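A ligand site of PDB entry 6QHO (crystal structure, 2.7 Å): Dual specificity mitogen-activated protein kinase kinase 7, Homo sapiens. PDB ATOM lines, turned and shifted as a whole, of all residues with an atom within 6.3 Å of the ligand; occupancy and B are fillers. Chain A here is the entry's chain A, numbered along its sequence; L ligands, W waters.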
ATOM      1  N   MET A  36     -17.245  15.506 -20.350  1.00  0.00           N
ATOM      2  CA  MET A  36     -15.924  14.939 -20.070  1.00  0.00           C
ATOM      3  C   MET A  36     -14.885  15.864 -20.674  1.00  0.00           C
ATOM      4  O   MET A  36     -14.807  16.007 -21.901  1.00  0.00           O
ATOM      5  CB  MET A  36     -15.809  13.527 -20.629  1.00  0.00           C
ATOM      6  CG  MET A  36     -16.936  12.622 -20.180  1.00  0.00           C
ATOM      7  SD  MET A  36     -16.560  10.877 -20.341  1.00  0.00           S
ATOM      8  CE  MET A  36     -16.808  10.651 -22.094  1.00  0.00           C
ATOM      9  N   GLY A  37     -14.096  16.506 -19.814  1.00  0.00           N
ATOM     10  CA  GLY A  37     -12.976  17.305 -20.283  1.00  0.00           C
ATOM     11  C   GLY A  37     -13.406  18.434 -21.185  1.00  0.00           C
ATOM     12  O   GLY A  37     -14.463  19.047 -20.992  1.00  0.00           O
ATOM     13  N   SER A  38     -12.591  18.712 -22.205  1.00  0.00           N
ATOM     14  CA  SER A  38     -12.803  19.809 -23.134  1.00  0.00           C
ATOM     15  C   SER A  38     -13.221  19.300 -24.505  1.00  0.00           C
ATOM     16  O   SER A  38     -13.132  18.110 -24.807  1.00  0.00           O
ATOM     17  CB  SER A  38     -11.538  20.661 -23.249  1.00  0.00           C
ATOM     18  OG  SER A  38     -11.820  21.946 -23.765  1.00  0.00           O
ATOM     19  N   GLY A  39     -13.694  20.224 -25.335  1.00  0.00           N
ATOM     20  CA  GLY A  39     -14.039  19.893 -26.703  1.00  0.00           C
ATOM     21  C   GLY A  39     -12.848  20.001 -27.619  1.00  0.00           C
ATOM     22  O   GLY A  39     -12.766  20.925 -28.434  1.00  0.00           O
ATOM     23  N   THR A  40     -11.897  19.060 -27.504  1.00  0.00           N
ATOM     24  CA  THR A  40     -10.701  19.124 -28.330  1.00  0.00           C
ATOM     25  C   THR A  40     -11.017  18.797 -29.786  1.00  0.00           C
ATOM     26  O   THR A  40     -10.453  19.404 -30.704  1.00  0.00           O
ATOM     27  CB  THR A  40      -9.606  18.199 -27.773  1.00  0.00           C
ATOM     28  OG1 THR A  40      -8.334  18.591 -28.299  1.00  0.00           O
ATOM     29  CG2 THR A  40      -9.870  16.723 -28.086  1.00  0.00           C
ATOM     30  N   GLY A  42     -14.764  17.452 -30.349  1.00  0.00           N
ATOM     31  CA  GLY A  42     -16.131  17.886 -30.124  1.00  0.00           C
ATOM     32  C   GLY A  42     -16.462  17.871 -28.641  1.00  0.00           C
ATOM     33  O   GLY A  42     -15.676  17.429 -27.803  1.00  0.00           O
ATOM     34  N   VAL A  44     -17.939  16.206 -25.697  1.00  0.00           N
ATOM     35  CA  VAL A  44     -18.144  14.789 -25.377  1.00  0.00           C
ATOM     36  C   VAL A  44     -18.845  14.669 -24.028  1.00  0.00           C
ATOM     37  O   VAL A  44     -18.326  15.116 -22.995  1.00  0.00           O
ATOM     38  CB  VAL A  44     -16.823  14.007 -25.380  1.00  0.00           C
ATOM     39  CG1 VAL A  44     -17.110  12.552 -25.127  1.00  0.00           C
ATOM     40  CG2 VAL A  44     -16.102  14.175 -26.698  1.00  0.00           C
ATOM     41  N   ALA A  57     -19.638   7.168 -23.921  1.00  0.00           N
ATOM     42  CA  ALA A  57     -19.233   8.496 -24.359  1.00  0.00           C
ATOM     43  C   ALA A  57     -20.025   8.856 -25.603  1.00  0.00           C
ATOM     44  O   ALA A  57     -20.141   8.042 -26.534  1.00  0.00           O
ATOM     45  CB  ALA A  57     -17.737   8.538 -24.642  1.00  0.00           C
ATOM     46  N   LYS A  59     -20.251  11.992 -28.403  1.00  0.00           N
ATOM     47  CA  LYS A  59     -19.830  13.275 -28.945  1.00  0.00           C
ATOM     48  C   LYS A  59     -21.008  13.920 -29.644  1.00  0.00           C
ATOM     49  O   LYS A  59     -21.777  13.251 -30.344  1.00  0.00           O
ATOM     50  CB  LYS A  59     -18.656  13.092 -29.906  1.00  0.00           C
ATOM     51  CG  LYS A  59     -17.972  14.396 -30.297  1.00  0.00           C
ATOM     52  CD  LYS A  59     -16.982  14.189 -31.431  1.00  0.00           C
ATOM     53  CE  LYS A  59     -15.911  13.158 -31.058  1.00  0.00           C
ATOM     54  NZ  LYS A  59     -14.983  12.887 -32.193  1.00  0.00           N
ATOM     55  N   VAL A  90     -10.467   3.298 -30.677  1.00  0.00           N
ATOM     56  CA  VAL A  90     -11.744   3.329 -29.956  1.00  0.00           C
ATOM     57  C   VAL A  90     -12.887   3.083 -30.931  1.00  0.00           C
ATOM     58  O   VAL A  90     -12.962   3.688 -32.010  1.00  0.00           O
ATOM     59  CB  VAL A  90     -11.917   4.651 -29.200  1.00  0.00           C
ATOM     60  CG1 VAL A  90     -11.183   4.599 -27.871  1.00  0.00           C
ATOM     61  CG2 VAL A  90     -11.438   5.819 -30.031  1.00  0.00           C
ATOM     62  N   MET A 106     -19.572   6.524 -28.592  1.00  0.00           N
ATOM     63  CA  MET A 106     -18.284   5.854 -28.467  1.00  0.00           C
ATOM     64  C   MET A 106     -18.236   5.028 -27.192  1.00  0.00           C
ATOM     65  O   MET A 106     -18.871   5.370 -26.188  1.00  0.00           O
ATOM     66  CB  MET A 106     -17.121   6.868 -28.452  1.00  0.00           C
ATOM     67  CG  MET A 106     -17.159   7.927 -29.530  1.00  0.00           C
ATOM     68  SD  MET A 106     -16.882   7.275 -31.188  1.00  0.00           S
ATOM     69  CE  MET A 106     -15.318   6.438 -30.959  1.00  0.00           C
ATOM     70  N   GLU A 107     -17.460   3.948 -27.229  1.00  0.00           N
ATOM     71  CA  GLU A 107     -17.176   3.216 -26.009  1.00  0.00           C
ATOM     72  C   GLU A 107     -16.467   4.130 -25.024  1.00  0.00           C
ATOM     73  O   GLU A 107     -15.597   4.929 -25.396  1.00  0.00           O
ATOM     74  CB  GLU A 107     -16.319   1.979 -26.317  1.00  0.00           C
ATOM     75  CG  GLU A 107     -14.928   2.260 -26.826  1.00  0.00           C
ATOM     76  CD  GLU A 107     -14.046   1.012 -26.849  1.00  0.00           C
ATOM     77  OE1 GLU A 107     -14.222   0.143 -25.964  1.00  0.00           O
ATOM     78  OE2 GLU A 107     -13.191   0.905 -27.754  1.00  0.00           O
ATOM     79  N   LEU A 108     -16.869   4.050 -23.759  1.00  0.00           N
ATOM     80  CA  LEU A 108     -16.341   4.933 -22.733  1.00  0.00           C
ATOM     81  C   LEU A 108     -14.962   4.458 -22.309  1.00  0.00           C
ATOM     82  O   LEU A 108     -14.795   3.301 -21.912  1.00  0.00           O
ATOM     83  CB  LEU A 108     -17.310   4.979 -21.541  1.00  0.00           C
ATOM     84  CG  LEU A 108     -17.073   5.987 -20.412  1.00  0.00           C
ATOM     85  CD1 LEU A 108     -16.421   7.248 -20.924  1.00  0.00           C
ATOM     86  CD2 LEU A 108     -18.395   6.307 -19.777  1.00  0.00           C
ATOM     87  N   MET A 109     -13.972   5.336 -22.409  1.00  0.00           N
ATOM     88  CA  MET A 109     -12.647   5.051 -21.869  1.00  0.00           C
ATOM     89  C   MET A 109     -12.503   5.763 -20.525  1.00  0.00           C
ATOM     90  O   MET A 109     -13.430   6.426 -20.046  1.00  0.00           O
ATOM     91  CB  MET A 109     -11.554   5.476 -22.852  1.00  0.00           C
ATOM     92  CG  MET A 109     -11.546   4.714 -24.183  1.00  0.00           C
ATOM     93  SD  MET A 109     -11.309   2.927 -24.057  1.00  0.00           S
ATOM     94  CE  MET A 109      -9.589   2.818 -23.581  1.00  0.00           C
ATOM     95  N   GLY A 110     -11.337   5.596 -19.898  1.00  0.00           N
ATOM     96  CA  GLY A 110     -11.133   6.166 -18.575  1.00  0.00           C
ATOM     97  C   GLY A 110     -10.668   7.606 -18.629  1.00  0.00           C
ATOM     98  O   GLY A 110     -11.389   8.519 -18.221  1.00  0.00           O
ATOM     99  N   THR A 111      -9.459   7.797 -19.132  1.00  0.00           N
ATOM    100  CA  THR A 111      -8.864   9.122 -19.338  1.00  0.00           C
ATOM    101  C   THR A 111      -7.657   8.937 -20.244  1.00  0.00           C
ATOM    102  O   THR A 111      -7.431   7.842 -20.779  1.00  0.00           O
ATOM    103  CB  THR A 111      -8.512   9.786 -18.006  1.00  0.00           C
ATOM    104  OG1 THR A 111      -8.108  11.144 -18.239  1.00  0.00           O
ATOM    105  CG2 THR A 111      -7.392   9.042 -17.299  1.00  0.00           C
ATOM    106  N   CYS A 112      -6.878   9.981 -20.431  1.00  0.00           N
ATOM    107  CA  CYS A 112      -5.732   9.937 -21.316  1.00  0.00           C
ATOM    108  C   CYS A 112      -4.441   9.852 -20.517  1.00  0.00           C
ATOM    109  O   CYS A 112      -4.406  10.101 -19.302  1.00  0.00           O
ATOM    110  CB  CYS A 112      -5.713  11.145 -22.253  1.00  0.00           C
ATOM    111  SG  CYS A 112      -5.674  12.709 -21.400  1.00  0.00           S
ATOM    112  N   ALA A 113      -3.366   9.505 -21.222  1.00  0.00           N
ATOM    113  CA  ALA A 113      -2.062   9.408 -20.582  1.00  0.00           C
ATOM    114  C   ALA A 113      -1.610  10.751 -20.023  1.00  0.00           C
ATOM    115  O   ALA A 113      -0.883  10.786 -19.015  1.00  0.00           O
ATOM    116  CB  ALA A 113      -1.031   8.871 -21.580  1.00  0.00           C
ATOM    117  N   GLU A 114      -2.024  11.860 -20.636  1.00  0.00           N
ATOM    118  CA  GLU A 114      -1.674  13.166 -20.098  1.00  0.00           C
ATOM    119  C   GLU A 114      -2.194  13.345 -18.685  1.00  0.00           C
ATOM    120  O   GLU A 114      -1.487  13.840 -17.803  1.00  0.00           O
ATOM    121  CB  GLU A 114      -2.207  14.277 -21.005  1.00  0.00           C
ATOM    122  CG  GLU A 114      -1.432  15.578 -20.907  1.00  0.00           C
ATOM    123  CD  GLU A 114      -2.171  16.661 -20.140  1.00  0.00           C
ATOM    124  OE1 GLU A 114      -1.551  17.273 -19.233  1.00  0.00           O
ATOM    125  OE2 GLU A 114      -3.358  16.894 -20.440  1.00  0.00           O
ATOM    126  N   LYS A 115      -3.440  12.918 -18.432  1.00  0.00           N
ATOM    127  CA  LYS A 115      -4.033  13.113 -17.119  1.00  0.00           C
ATOM    128  C   LYS A 115      -3.564  12.070 -16.110  1.00  0.00           C
ATOM    129  O   LYS A 115      -3.484  12.369 -14.918  1.00  0.00           O
ATOM    130  CB  LYS A 115      -5.555  13.121 -17.233  1.00  0.00           C
ATOM    131  CG  LYS A 115      -6.125  14.534 -17.313  1.00  0.00           C
ATOM    132  CD  LYS A 115      -7.332  14.639 -18.223  1.00  0.00           C
ATOM    133  CE  LYS A 115      -7.378  15.995 -18.916  1.00  0.00           C
ATOM    134  NZ  LYS A 115      -8.714  16.273 -19.545  1.00  0.00           N
ATOM    135  N   PRO A 156       0.286  12.357 -25.717  1.00  0.00           N
ATOM    136  CA  PRO A 156      -0.317  11.647 -24.580  1.00  0.00           C
ATOM    137  C   PRO A 156      -1.810  11.905 -24.365  1.00  0.00           C
ATOM    138  O   PRO A 156      -2.498  11.030 -23.836  1.00  0.00           O
ATOM    139  CB  PRO A 156       0.511  12.131 -23.391  1.00  0.00           C
ATOM    140  CG  PRO A 156       1.832  12.471 -23.979  1.00  0.00           C
ATOM    141  CD  PRO A 156       1.520  13.062 -25.320  1.00  0.00           C
ATOM    142  N   SER A 157      -2.326  13.073 -24.747  1.00  0.00           N
ATOM    143  CA  SER A 157      -3.756  13.294 -24.593  1.00  0.00           C
ATOM    144  C   SER A 157      -4.588  12.458 -25.559  1.00  0.00           C
ATOM    145  O   SER A 157      -5.796  12.303 -25.345  1.00  0.00           O
ATOM    146  CB  SER A 157      -4.090  14.777 -24.780  1.00  0.00           C
ATOM    147  OG  SER A 157      -3.748  15.212 -26.082  1.00  0.00           O
ATOM    148  N   ASN A 158      -3.977  11.896 -26.601  1.00  0.00           N
ATOM    149  CA  ASN A 158      -4.682  11.067 -27.571  1.00  0.00           C
ATOM    150  C   ASN A 158      -4.606   9.572 -27.259  1.00  0.00           C
ATOM    151  O   ASN A 158      -5.233   8.776 -27.965  1.00  0.00           O
ATOM    152  CB  ASN A 158      -4.147  11.338 -28.973  1.00  0.00           C
ATOM    153  CG  ASN A 158      -4.668  12.640 -29.548  1.00  0.00           C
ATOM    154  OD1 ASN A 158      -5.668  13.179 -29.050  1.00  0.00           O
ATOM    155  ND2 ASN A 158      -4.001  13.153 -30.572  1.00  0.00           N
ATOM    156  N   ILE A 159      -3.861   9.186 -26.237  1.00  0.00           N
ATOM    157  CA  ILE A 159      -3.776   7.796 -25.809  1.00  0.00           C
ATOM    158  C   ILE A 159      -4.754   7.632 -24.668  1.00  0.00           C
ATOM    159  O   ILE A 159      -4.565   8.197 -23.592  1.00  0.00           O
ATOM    160  CB  ILE A 159      -2.356   7.419 -25.392  1.00  0.00           C
ATOM    161  CG1 ILE A 159      -1.423   7.414 -26.610  1.00  0.00           C
ATOM    162  CG2 ILE A 159      -2.344   6.077 -24.658  1.00  0.00           C
ATOM    163  CD1 ILE A 159      -0.109   8.143 -26.373  1.00  0.00           C
ATOM    164  N   LEU A 160      -5.811   6.857 -24.887  1.00  0.00           N
ATOM    165  CA  LEU A 160      -6.804   6.615 -23.851  1.00  0.00           C
ATOM    166  C   LEU A 160      -6.615   5.244 -23.216  1.00  0.00           C
ATOM    167  O   LEU A 160      -6.170   4.299 -23.877  1.00  0.00           O
ATOM    168  CB  LEU A 160      -8.229   6.728 -24.419  1.00  0.00           C
ATOM    169  CG  LEU A 160      -8.557   8.025 -25.173  1.00  0.00           C
ATOM    170  CD1 LEU A 160     -10.053   8.123 -25.445  1.00  0.00           C
ATOM    171  CD2 LEU A 160      -8.088   9.242 -24.401  1.00  0.00           C
ATOM    172  N   CYS A 170      -7.300   7.619 -30.267  1.00  0.00           N
ATOM    173  CA  CYS A 170      -8.657   8.173 -30.229  1.00  0.00           C
ATOM    174  C   CYS A 170      -8.989   9.356 -31.134  1.00  0.00           C
ATOM    175  O   CYS A 170     -10.182   9.544 -31.421  1.00  0.00           O
ATOM    176  CB  CYS A 170      -9.009   8.575 -28.797  1.00  0.00           C
ATOM    177  SG  CYS A 170      -8.312  10.141 -28.291  1.00  0.00           S
HETATM  178  C1  LIG L   1     -12.883  10.507 -24.078  1.00  0.00           C
HETATM  179  C2  LIG L   1     -13.331   9.791 -25.276  1.00  0.00           C
HETATM  180  C3  LIG L   1     -13.885   8.431 -25.039  1.00  0.00           C
HETATM  181  N1  LIG L   1     -13.918   7.968 -23.767  1.00  0.00           N
HETATM  182  C4  LIG L   1     -13.471   8.699 -22.733  1.00  0.00           C
HETATM  183  O1  LIG L   1      -9.170  15.159 -21.720  1.00  0.00           O
HETATM  184  C5  LIG L   1      -9.121  14.243 -22.521  1.00  0.00           C
HETATM  185  C6  LIG L   1      -8.119  13.139 -22.355  1.00  0.00           C
HETATM  186  C7  LIG L   1      -6.764  13.804 -22.222  1.00  0.00           C
HETATM  187  C8  LIG L   1     -13.149  10.597 -26.451  1.00  0.00           C
HETATM  188  C9  LIG L   1     -11.854  12.864 -23.916  1.00  0.00           C
HETATM  189  C10 LIG L   1     -12.574  14.128 -24.393  1.00  0.00           C
HETATM  190  C11 LIG L   1     -11.933  15.365 -23.797  1.00  0.00           C
HETATM  191  C12 LIG L   1     -10.454  15.407 -24.173  1.00  0.00           C
HETATM  192  C13 LIG L   1     -10.361  12.965 -24.227  1.00  0.00           C
HETATM  193  N2  LIG L   1     -12.971   9.935 -22.857  1.00  0.00           N
HETATM  194  N3  LIG L   1     -12.452  11.672 -24.574  1.00  0.00           N
HETATM  195  N4  LIG L   1     -12.594  11.752 -25.978  1.00  0.00           N
HETATM  196  N5  LIG L   1     -14.334   7.670 -26.068  1.00  0.00           N
HETATM  197  N6  LIG L   1      -9.930  14.190 -23.582  1.00  0.00           N
HETATM  198  O   HOH W   1     -11.985  11.277 -20.033  1.00  0.00           O
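SG of Cys 112 lies within hydrogen-bond range of N of Lys 115, 3.7 Å away.
N of Met 36 is in hydrogen-bond range of O of Val 44 (2.9 Å).
N of Met 106 sits at hydrogen-bond distance from O of Ala 57 (2.6 Å).
Residues that only touch the ligand: Met 36, Ser 38, Ala 57, Met 106, Leu 108, Ser 157 and Leu 160.
Hydrophobic or aromatic side chains within 4 Å of the ligand: Met 36, Ala 57, Met 106, Leu 108, Met 109 and Leu 160.
Within 4 Å of the ligand: Met 36, Ser 38, Ala 57, Met 106, Glu 107, Leu 108, Met 109, Cys 112, Lys 115, Ser 157 and Leu 160.
Water W1 lies within hydrogen-bond range of a nitrogen (N2) of the ligand (3.3 Å) and the backbone carbonyl oxygen (O) of Gly 110 (3.4 Å).
A carbon (C7) of the ligand is bonded to the side-chain sulfur (SG) of Cys 112 (1.8 Å).
The side-chain amino group (NZ) of Lys 115 is in hydrogen-bond range of an oxygen (O1) of the ligand (2.5 Å).
N of Met 109 sits at hydrogen-bond distance from N1 of the ligand (3.0 Å).
The backbone carbonyl oxygen (O) of Glu 107 sits at hydrogen-bond distance from a nitrogen (N5) of the ligand (3.1 Å).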
